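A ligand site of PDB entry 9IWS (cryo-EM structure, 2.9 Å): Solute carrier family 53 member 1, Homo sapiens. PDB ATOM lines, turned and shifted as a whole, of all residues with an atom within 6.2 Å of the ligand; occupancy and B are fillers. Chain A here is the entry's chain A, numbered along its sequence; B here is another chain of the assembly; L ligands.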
ATOM      1  N   MET A   1      25.591  -2.149 -20.056  1.00  0.00           N
ATOM      2  CA  MET A   1      24.493  -2.864 -20.685  1.00  0.00           C
ATOM      3  C   MET A   1      23.200  -2.067 -20.680  1.00  0.00           C
ATOM      4  O   MET A   1      22.612  -1.800 -21.721  1.00  0.00           O
ATOM      5  CB  MET A   1      24.295  -4.237 -20.028  1.00  0.00           C
ATOM      6  CG  MET A   1      23.243  -5.164 -20.672  1.00  0.00           C
ATOM      7  SD  MET A   1      22.839  -4.925 -22.428  1.00  0.00           S
ATOM      8  CE  MET A   1      24.430  -4.630 -23.201  1.00  0.00           C
ATOM      9  N   LYS A   2      22.774  -1.682 -19.482  1.00  0.00           N
ATOM     10  CA  LYS A   2      21.572  -0.869 -19.304  1.00  0.00           C
ATOM     11  C   LYS A   2      22.018   0.457 -18.693  1.00  0.00           C
ATOM     12  O   LYS A   2      22.211   0.564 -17.486  1.00  0.00           O
ATOM     13  CB  LYS A   2      20.559  -1.592 -18.417  1.00  0.00           C
ATOM     14  CG  LYS A   2      19.996  -2.867 -18.998  1.00  0.00           C
ATOM     15  CD  LYS A   2      19.684  -2.707 -20.475  1.00  0.00           C
ATOM     16  CE  LYS A   2      18.314  -3.272 -20.813  1.00  0.00           C
ATOM     17  NZ  LYS A   2      17.713  -2.599 -22.003  1.00  0.00           N
ATOM     18  N   PHE A   3      22.210   1.466 -19.548  1.00  0.00           N
ATOM     19  CA  PHE A   3      22.722   2.742 -19.071  1.00  0.00           C
ATOM     20  C   PHE A   3      21.641   3.642 -18.498  1.00  0.00           C
ATOM     21  O   PHE A   3      21.964   4.559 -17.727  1.00  0.00           O
ATOM     22  CB  PHE A   3      23.437   3.471 -20.216  1.00  0.00           C
ATOM     23  CG  PHE A   3      24.215   4.671 -19.768  1.00  0.00           C
ATOM     24  CD1 PHE A   3      25.241   4.547 -18.851  1.00  0.00           C
ATOM     25  CD2 PHE A   3      23.923   5.931 -20.261  1.00  0.00           C
ATOM     26  CE1 PHE A   3      25.960   5.650 -18.430  1.00  0.00           C
ATOM     27  CE2 PHE A   3      24.631   7.041 -19.848  1.00  0.00           C
ATOM     28  CZ  PHE A   3      25.649   6.901 -18.933  1.00  0.00           C
ATOM     29  N   ALA A   4      20.373   3.411 -18.841  1.00  0.00           N
ATOM     30  CA  ALA A   4      19.317   4.333 -18.435  1.00  0.00           C
ATOM     31  C   ALA A   4      19.146   4.361 -16.922  1.00  0.00           C
ATOM     32  O   ALA A   4      19.205   5.442 -16.306  1.00  0.00           O
ATOM     33  CB  ALA A   4      18.009   3.952 -19.121  1.00  0.00           C
ATOM     34  N   TYR A  22      19.498  11.635 -21.633  1.00  0.00           N
ATOM     35  CA  TYR A  22      19.729  10.406 -22.374  1.00  0.00           C
ATOM     36  C   TYR A  22      18.419   9.837 -22.921  1.00  0.00           C
ATOM     37  O   TYR A  22      18.334   9.446 -24.089  1.00  0.00           O
ATOM     38  CB  TYR A  22      20.447   9.392 -21.491  1.00  0.00           C
ATOM     39  CG  TYR A  22      20.939   8.161 -22.204  1.00  0.00           C
ATOM     40  CD1 TYR A  22      22.075   8.212 -23.000  1.00  0.00           C
ATOM     41  CD2 TYR A  22      20.279   6.947 -22.067  1.00  0.00           C
ATOM     42  CE1 TYR A  22      22.532   7.083 -23.657  1.00  0.00           C
ATOM     43  CE2 TYR A  22      20.729   5.815 -22.718  1.00  0.00           C
ATOM     44  CZ  TYR A  22      21.861   5.886 -23.505  1.00  0.00           C
ATOM     45  OH  TYR A  22      22.313   4.765 -24.148  1.00  0.00           O
ATOM     46  N   LYS A  26      17.165   9.055 -26.745  1.00  0.00           N
ATOM     47  CA  LYS A  26      16.775   7.715 -27.175  1.00  0.00           C
ATOM     48  C   LYS A  26      15.398   7.725 -27.825  1.00  0.00           C
ATOM     49  O   LYS A  26      15.186   7.116 -28.879  1.00  0.00           O
ATOM     50  CB  LYS A  26      16.795   6.754 -25.979  1.00  0.00           C
ATOM     51  CG  LYS A  26      18.080   5.978 -25.819  1.00  0.00           C
ATOM     52  CD  LYS A  26      17.835   4.636 -25.162  1.00  0.00           C
ATOM     53  CE  LYS A  26      16.990   4.781 -23.913  1.00  0.00           C
ATOM     54  NZ  LYS A  26      16.485   3.472 -23.423  1.00  0.00           N
ATOM     55  N   TYR A  30      14.484   6.829 -31.732  1.00  0.00           N
ATOM     56  CA  TYR A  30      13.519   5.797 -32.072  1.00  0.00           C
ATOM     57  C   TYR A  30      12.388   6.350 -32.938  1.00  0.00           C
ATOM     58  O   TYR A  30      11.948   5.709 -33.893  1.00  0.00           O
ATOM     59  CB  TYR A  30      12.960   5.142 -30.809  1.00  0.00           C
ATOM     60  CG  TYR A  30      13.921   4.175 -30.158  1.00  0.00           C
ATOM     61  CD1 TYR A  30      15.053   3.733 -30.828  1.00  0.00           C
ATOM     62  CD2 TYR A  30      13.691   3.699 -28.873  1.00  0.00           C
ATOM     63  CE1 TYR A  30      15.930   2.838 -30.241  1.00  0.00           C
ATOM     64  CE2 TYR A  30      14.567   2.803 -28.272  1.00  0.00           C
ATOM     65  CZ  TYR A  30      15.680   2.387 -28.963  1.00  0.00           C
ATOM     66  OH  TYR A  30      16.552   1.501 -28.376  1.00  0.00           O
ATOM     67  N   ARG A 157      29.287   9.622 -24.865  1.00  0.00           N
ATOM     68  CA  ARG A 157      29.868   8.578 -25.704  1.00  0.00           C
ATOM     69  C   ARG A 157      28.861   7.478 -26.004  1.00  0.00           C
ATOM     70  O   ARG A 157      28.752   7.017 -27.145  1.00  0.00           O
ATOM     71  CB  ARG A 157      31.107   8.001 -25.024  1.00  0.00           C
ATOM     72  CG  ARG A 157      31.613   6.705 -25.650  1.00  0.00           C
ATOM     73  CD  ARG A 157      32.575   5.983 -24.720  1.00  0.00           C
ATOM     74  NE  ARG A 157      31.903   4.945 -23.942  1.00  0.00           N
ATOM     75  CZ  ARG A 157      31.502   3.783 -24.421  1.00  0.00           C
ATOM     76  NH1 ARG A 157      31.690   3.459 -25.696  1.00  0.00           N
ATOM     77  NH2 ARG A 157      30.907   2.918 -23.613  1.00  0.00           N
ATOM     78  N   LYS A 158      28.101   7.058 -24.992  1.00  0.00           N
ATOM     79  CA  LYS A 158      27.153   5.960 -25.195  1.00  0.00           C
ATOM     80  C   LYS A 158      26.022   6.359 -26.138  1.00  0.00           C
ATOM     81  O   LYS A 158      25.625   5.579 -27.003  1.00  0.00           O
ATOM     82  CB  LYS A 158      26.603   5.487 -23.857  1.00  0.00           C
ATOM     83  CG  LYS A 158      27.058   4.092 -23.477  1.00  0.00           C
ATOM     84  CD  LYS A 158      27.228   3.925 -21.983  1.00  0.00           C
ATOM     85  CE  LYS A 158      28.049   2.688 -21.667  1.00  0.00           C
ATOM     86  NZ  LYS A 158      27.657   2.073 -20.372  1.00  0.00           N
ATOM     87  N   LYS A 161      27.394   6.432 -29.677  1.00  0.00           N
ATOM     88  CA  LYS A 161      27.562   5.068 -30.186  1.00  0.00           C
ATOM     89  C   LYS A 161      26.213   4.471 -30.568  1.00  0.00           C
ATOM     90  O   LYS A 161      26.095   3.798 -31.607  1.00  0.00           O
ATOM     91  CB  LYS A 161      28.259   4.194 -29.142  1.00  0.00           C
ATOM     92  CG  LYS A 161      27.837   2.739 -29.164  1.00  0.00           C
ATOM     93  CD  LYS A 161      28.273   2.010 -27.900  1.00  0.00           C
ATOM     94  CE  LYS A 161      27.094   1.325 -27.236  1.00  0.00           C
ATOM     95  NZ  LYS A 161      26.710   0.069 -27.929  1.00  0.00           N
ATOM     96  N   LYS A 162      25.175   4.695 -29.754  1.00  0.00           N
ATOM     97  CA  LYS A 162      23.853   4.188 -30.082  1.00  0.00           C
ATOM     98  C   LYS A 162      23.323   4.823 -31.363  1.00  0.00           C
ATOM     99  O   LYS A 162      22.709   4.131 -32.186  1.00  0.00           O
ATOM    100  CB  LYS A 162      22.892   4.457 -28.916  1.00  0.00           C
ATOM    101  CG  LYS A 162      21.433   4.137 -29.232  1.00  0.00           C
ATOM    102  CD  LYS A 162      20.655   3.831 -27.961  1.00  0.00           C
ATOM    103  CE  LYS A 162      21.409   2.869 -27.069  1.00  0.00           C
ATOM    104  NZ  LYS A 162      20.719   2.651 -25.776  1.00  0.00           N
ATOM    105  N   LYS A 165      24.582   3.418 -34.873  1.00  0.00           N
ATOM    106  CA  LYS A 165      24.165   2.073 -35.256  1.00  0.00           C
ATOM    107  C   LYS A 165      22.845   2.061 -36.017  1.00  0.00           C
ATOM    108  O   LYS A 165      22.740   1.394 -37.054  1.00  0.00           O
ATOM    109  CB  LYS A 165      24.054   1.199 -34.005  1.00  0.00           C
ATOM    110  CG  LYS A 165      23.250  -0.073 -34.205  1.00  0.00           C
ATOM    111  CD  LYS A 165      23.584  -1.102 -33.140  1.00  0.00           C
ATOM    112  CE  LYS A 165      22.920  -0.767 -31.816  1.00  0.00           C
ATOM    113  NZ  LYS A 165      21.500  -1.219 -31.770  1.00  0.00           N
ATOM    114  N   ARG B 211      21.903  -9.842 -34.677  1.00  0.00           N
ATOM    115  CA  ARG B 211      22.853  -9.767 -33.577  1.00  0.00           C
ATOM    116  C   ARG B 211      22.188  -9.784 -32.214  1.00  0.00           C
ATOM    117  O   ARG B 211      22.849 -10.090 -31.214  1.00  0.00           O
ATOM    118  CB  ARG B 211      23.718  -8.505 -33.700  1.00  0.00           C
ATOM    119  CG  ARG B 211      25.140  -8.676 -33.197  1.00  0.00           C
ATOM    120  CD  ARG B 211      26.086  -7.715 -33.883  1.00  0.00           C
ATOM    121  NE  ARG B 211      27.453  -8.234 -33.957  1.00  0.00           N
ATOM    122  CZ  ARG B 211      28.272  -8.325 -32.924  1.00  0.00           C
ATOM    123  NH1 ARG B 211      27.924  -7.923 -31.712  1.00  0.00           N
ATOM    124  NH2 ARG B 211      29.490  -8.837 -33.109  1.00  0.00           N
ATOM    125  N   GLN B 212      20.887  -9.490 -32.141  1.00  0.00           N
ATOM    126  CA  GLN B 212      20.222  -9.334 -30.847  1.00  0.00           C
ATOM    127  C   GLN B 212      20.149 -10.658 -30.104  1.00  0.00           C
ATOM    128  O   GLN B 212      20.681 -10.800 -29.000  1.00  0.00           O
ATOM    129  CB  GLN B 212      18.830  -8.746 -31.047  1.00  0.00           C
ATOM    130  CG  GLN B 212      18.075  -8.490 -29.759  1.00  0.00           C
ATOM    131  CD  GLN B 212      17.444  -7.106 -29.712  1.00  0.00           C
ATOM    132  OE1 GLN B 212      17.817  -6.222 -30.478  1.00  0.00           O
ATOM    133  NE2 GLN B 212      16.494  -6.920 -28.809  1.00  0.00           N
ATOM    134  N   MET B 215      23.679 -12.280 -29.516  1.00  0.00           N
ATOM    135  CA  MET B 215      24.406 -11.657 -28.419  1.00  0.00           C
ATOM    136  C   MET B 215      23.769 -12.006 -27.084  1.00  0.00           C
ATOM    137  O   MET B 215      24.478 -12.275 -26.105  1.00  0.00           O
ATOM    138  CB  MET B 215      24.459 -10.144 -28.619  1.00  0.00           C
ATOM    139  CG  MET B 215      25.651  -9.680 -29.437  1.00  0.00           C
ATOM    140  SD  MET B 215      27.009 -10.862 -29.416  1.00  0.00           S
ATOM    141  CE  MET B 215      27.931 -10.312 -27.989  1.00  0.00           C
ATOM    142  N   LYS B 216      22.435 -12.021 -27.013  1.00  0.00           N
ATOM    143  CA  LYS B 216      21.760 -12.397 -25.768  1.00  0.00           C
ATOM    144  C   LYS B 216      22.140 -13.810 -25.354  1.00  0.00           C
ATOM    145  O   LYS B 216      22.343 -14.080 -24.158  1.00  0.00           O
ATOM    146  CB  LYS B 216      20.246 -12.269 -25.934  1.00  0.00           C
ATOM    147  CG  LYS B 216      19.431 -13.195 -25.035  1.00  0.00           C
ATOM    148  CD  LYS B 216      18.029 -12.656 -24.827  1.00  0.00           C
ATOM    149  CE  LYS B 216      17.351 -12.331 -26.154  1.00  0.00           C
ATOM    150  NZ  LYS B 216      16.980 -13.566 -26.901  1.00  0.00           N
ATOM    151  N   ARG B 219      25.880 -13.682 -24.056  1.00  0.00           N
ATOM    152  CA  ARG B 219      26.225 -12.816 -22.939  1.00  0.00           C
ATOM    153  C   ARG B 219      26.741 -13.634 -21.754  1.00  0.00           C
ATOM    154  O   ARG B 219      26.185 -14.681 -21.416  1.00  0.00           O
ATOM    155  CB  ARG B 219      25.031 -11.989 -22.502  1.00  0.00           C
ATOM    156  CG  ARG B 219      24.676 -10.842 -23.438  1.00  0.00           C
ATOM    157  CD  ARG B 219      25.476  -9.589 -23.126  1.00  0.00           C
ATOM    158  NE  ARG B 219      25.597  -8.737 -24.300  1.00  0.00           N
ATOM    159  CZ  ARG B 219      24.596  -8.086 -24.883  1.00  0.00           C
ATOM    160  NH1 ARG B 219      23.361  -8.160 -24.417  1.00  0.00           N
ATOM    161  NH2 ARG B 219      24.841  -7.333 -25.949  1.00  0.00           N
HETATM  162  C1  LIG L   1      23.259  -3.563 -27.114  1.00  0.00           C
HETATM  163  C2  LIG L   1      22.119  -2.635 -26.558  1.00  0.00           C
HETATM  164  C3  LIG L   1      22.547  -1.941 -25.214  1.00  0.00           C
HETATM  165  C4  LIG L   1      23.994  -1.422 -25.174  1.00  0.00           C
HETATM  166  C5  LIG L   1      24.923  -2.505 -25.704  1.00  0.00           C
HETATM  167  C6  LIG L   1      24.605  -2.846 -27.128  1.00  0.00           C
HETATM  168  O1  LIG L   1      23.016  -4.006 -28.405  1.00  0.00           O
HETATM  169  O2  LIG L   1      21.709  -1.707 -27.510  1.00  0.00           O
HETATM  170  O3  LIG L   1      21.701  -0.858 -24.962  1.00  0.00           O
HETATM  171  O4  LIG L   1      24.359  -1.177 -23.855  1.00  0.00           O
HETATM  172  O5  LIG L   1      26.245  -2.031 -25.620  1.00  0.00           O
HETATM  173  O6  LIG L   1      25.593  -3.737 -27.507  1.00  0.00           O
HETATM  174  O7  LIG L   1      23.635  -6.090 -29.906  1.00  0.00           O
HETATM  175  O8  LIG L   1      19.553  -0.303 -28.045  1.00  0.00           O
HETATM  176  O9  LIG L   1      19.087  -0.614 -25.040  1.00  0.00           O
HETATM  177  O10 LIG L   1      25.881   0.330 -22.309  1.00  0.00           O
HETATM  178  O11 LIG L   1      27.413  -4.346 -25.154  1.00  0.00           O
HETATM  179  O12 LIG L   1      28.055  -3.635 -28.265  1.00  0.00           O
HETATM  180  O13 LIG L   1      23.086  -6.457 -27.540  1.00  0.00           O
HETATM  181  O14 LIG L   1      20.120  -2.094 -29.630  1.00  0.00           O
HETATM  182  O15 LIG L   1      20.263  -0.008 -22.998  1.00  0.00           O
HETATM  183  O16 LIG L   1      23.461   0.787 -22.381  1.00  0.00           O
HETATM  184  O17 LIG L   1      27.676  -2.357 -23.485  1.00  0.00           O
HETATM  185  O18 LIG L   1      26.387  -1.934 -29.254  1.00  0.00           O
HETATM  186  O19 LIG L   1      21.257  -5.811 -29.143  1.00  0.00           O
HETATM  187  O20 LIG L   1      19.341  -2.700 -27.325  1.00  0.00           O
HETATM  188  O21 LIG L   1      20.155  -2.434 -23.561  1.00  0.00           O
HETATM  189  O22 LIG L   1      24.991   1.259 -24.396  1.00  0.00           O
HETATM  190  O23 LIG L   1      28.778  -2.336 -25.618  1.00  0.00           O
HETATM  191  O24 LIG L   1      26.364  -4.346 -29.909  1.00  0.00           O
HETATM  192  O25 LIG L   1      28.952   0.017 -24.708  1.00  0.00           O
HETATM  193  O26 LIG L   1      30.493  -1.598 -23.820  1.00  0.00           O
HETATM  194  O27 LIG L   1      30.862  -0.852 -26.166  1.00  0.00           O
HETATM  195  P1  LIG L   1      22.701  -5.603 -28.767  1.00  0.00           P
HETATM  196  P2  LIG L   1      20.147  -1.715 -28.133  1.00  0.00           P
HETATM  197  P3  LIG L   1      20.259  -1.034 -24.145  1.00  0.00           P
HETATM  198  P4  LIG L   1      24.672   0.362 -23.242  1.00  0.00           P
HETATM  199  P5  LIG L   1      27.451  -2.843 -24.879  1.00  0.00           P
HETATM  200  P6  LIG L   1      26.636  -3.383 -28.796  1.00  0.00           P
HETATM  201  P7  LIG L   1      29.791  -1.206 -25.165  1.00  0.00           P
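The side-chain amino group (NZ) of Lys 162 sits at hydrogen-bond distance from the side-chain hydroxyl (OH) of Tyr 22 (3.1 Å).
Residues that only touch the ligand: Tyr 30 (3.5 Å) and Gln 212 of chain B (3.7 Å). Within 4 Å of the ligand: Met 1, Lys 2, Phe 3, Tyr 30, Arg 157, Lys 158, Lys 161, Lys 162, Lys 165, Gln 212 of chain B and Arg 219 of chain B. Along chain A the residues within 4 Å of the ligand span positions 1 to 165.
The backbone NH of Met 1 is in hydrogen-bond range of an oxygen (O10) of the ligand (3.4 Å). O25 of the ligand is in salt-bridge range of NH2 of Arg 157. An oxygen (O10) of the ligand is in salt-bridge range of the side-chain amino group (NZ) of Lys 158, at 3.2 Å. An oxygen (O9) of the ligand lies within salt-bridge range of the side-chain amino group of Lys 162. The guanidinium group (NH2) of Arg 219 of chain B is in salt-bridge range of an oxygen (O13) of the ligand (2.5 Å). N of Phe 3 lies within hydrogen-bond range of O16 of the ligand. NZ of Lys 2 lies within salt-bridge range of O21 of the ligand, 2.9 Å away. O14 of the ligand lies within salt-bridge range of NZ of Lys 165, at 2.7 Å. O of Met 1 sits close to O16 of the ligand (2.8 Å). An oxygen (O18) of the ligand is in salt-bridge range of the side-chain amino group (NZ) of Lys 161 (2.4 Å).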
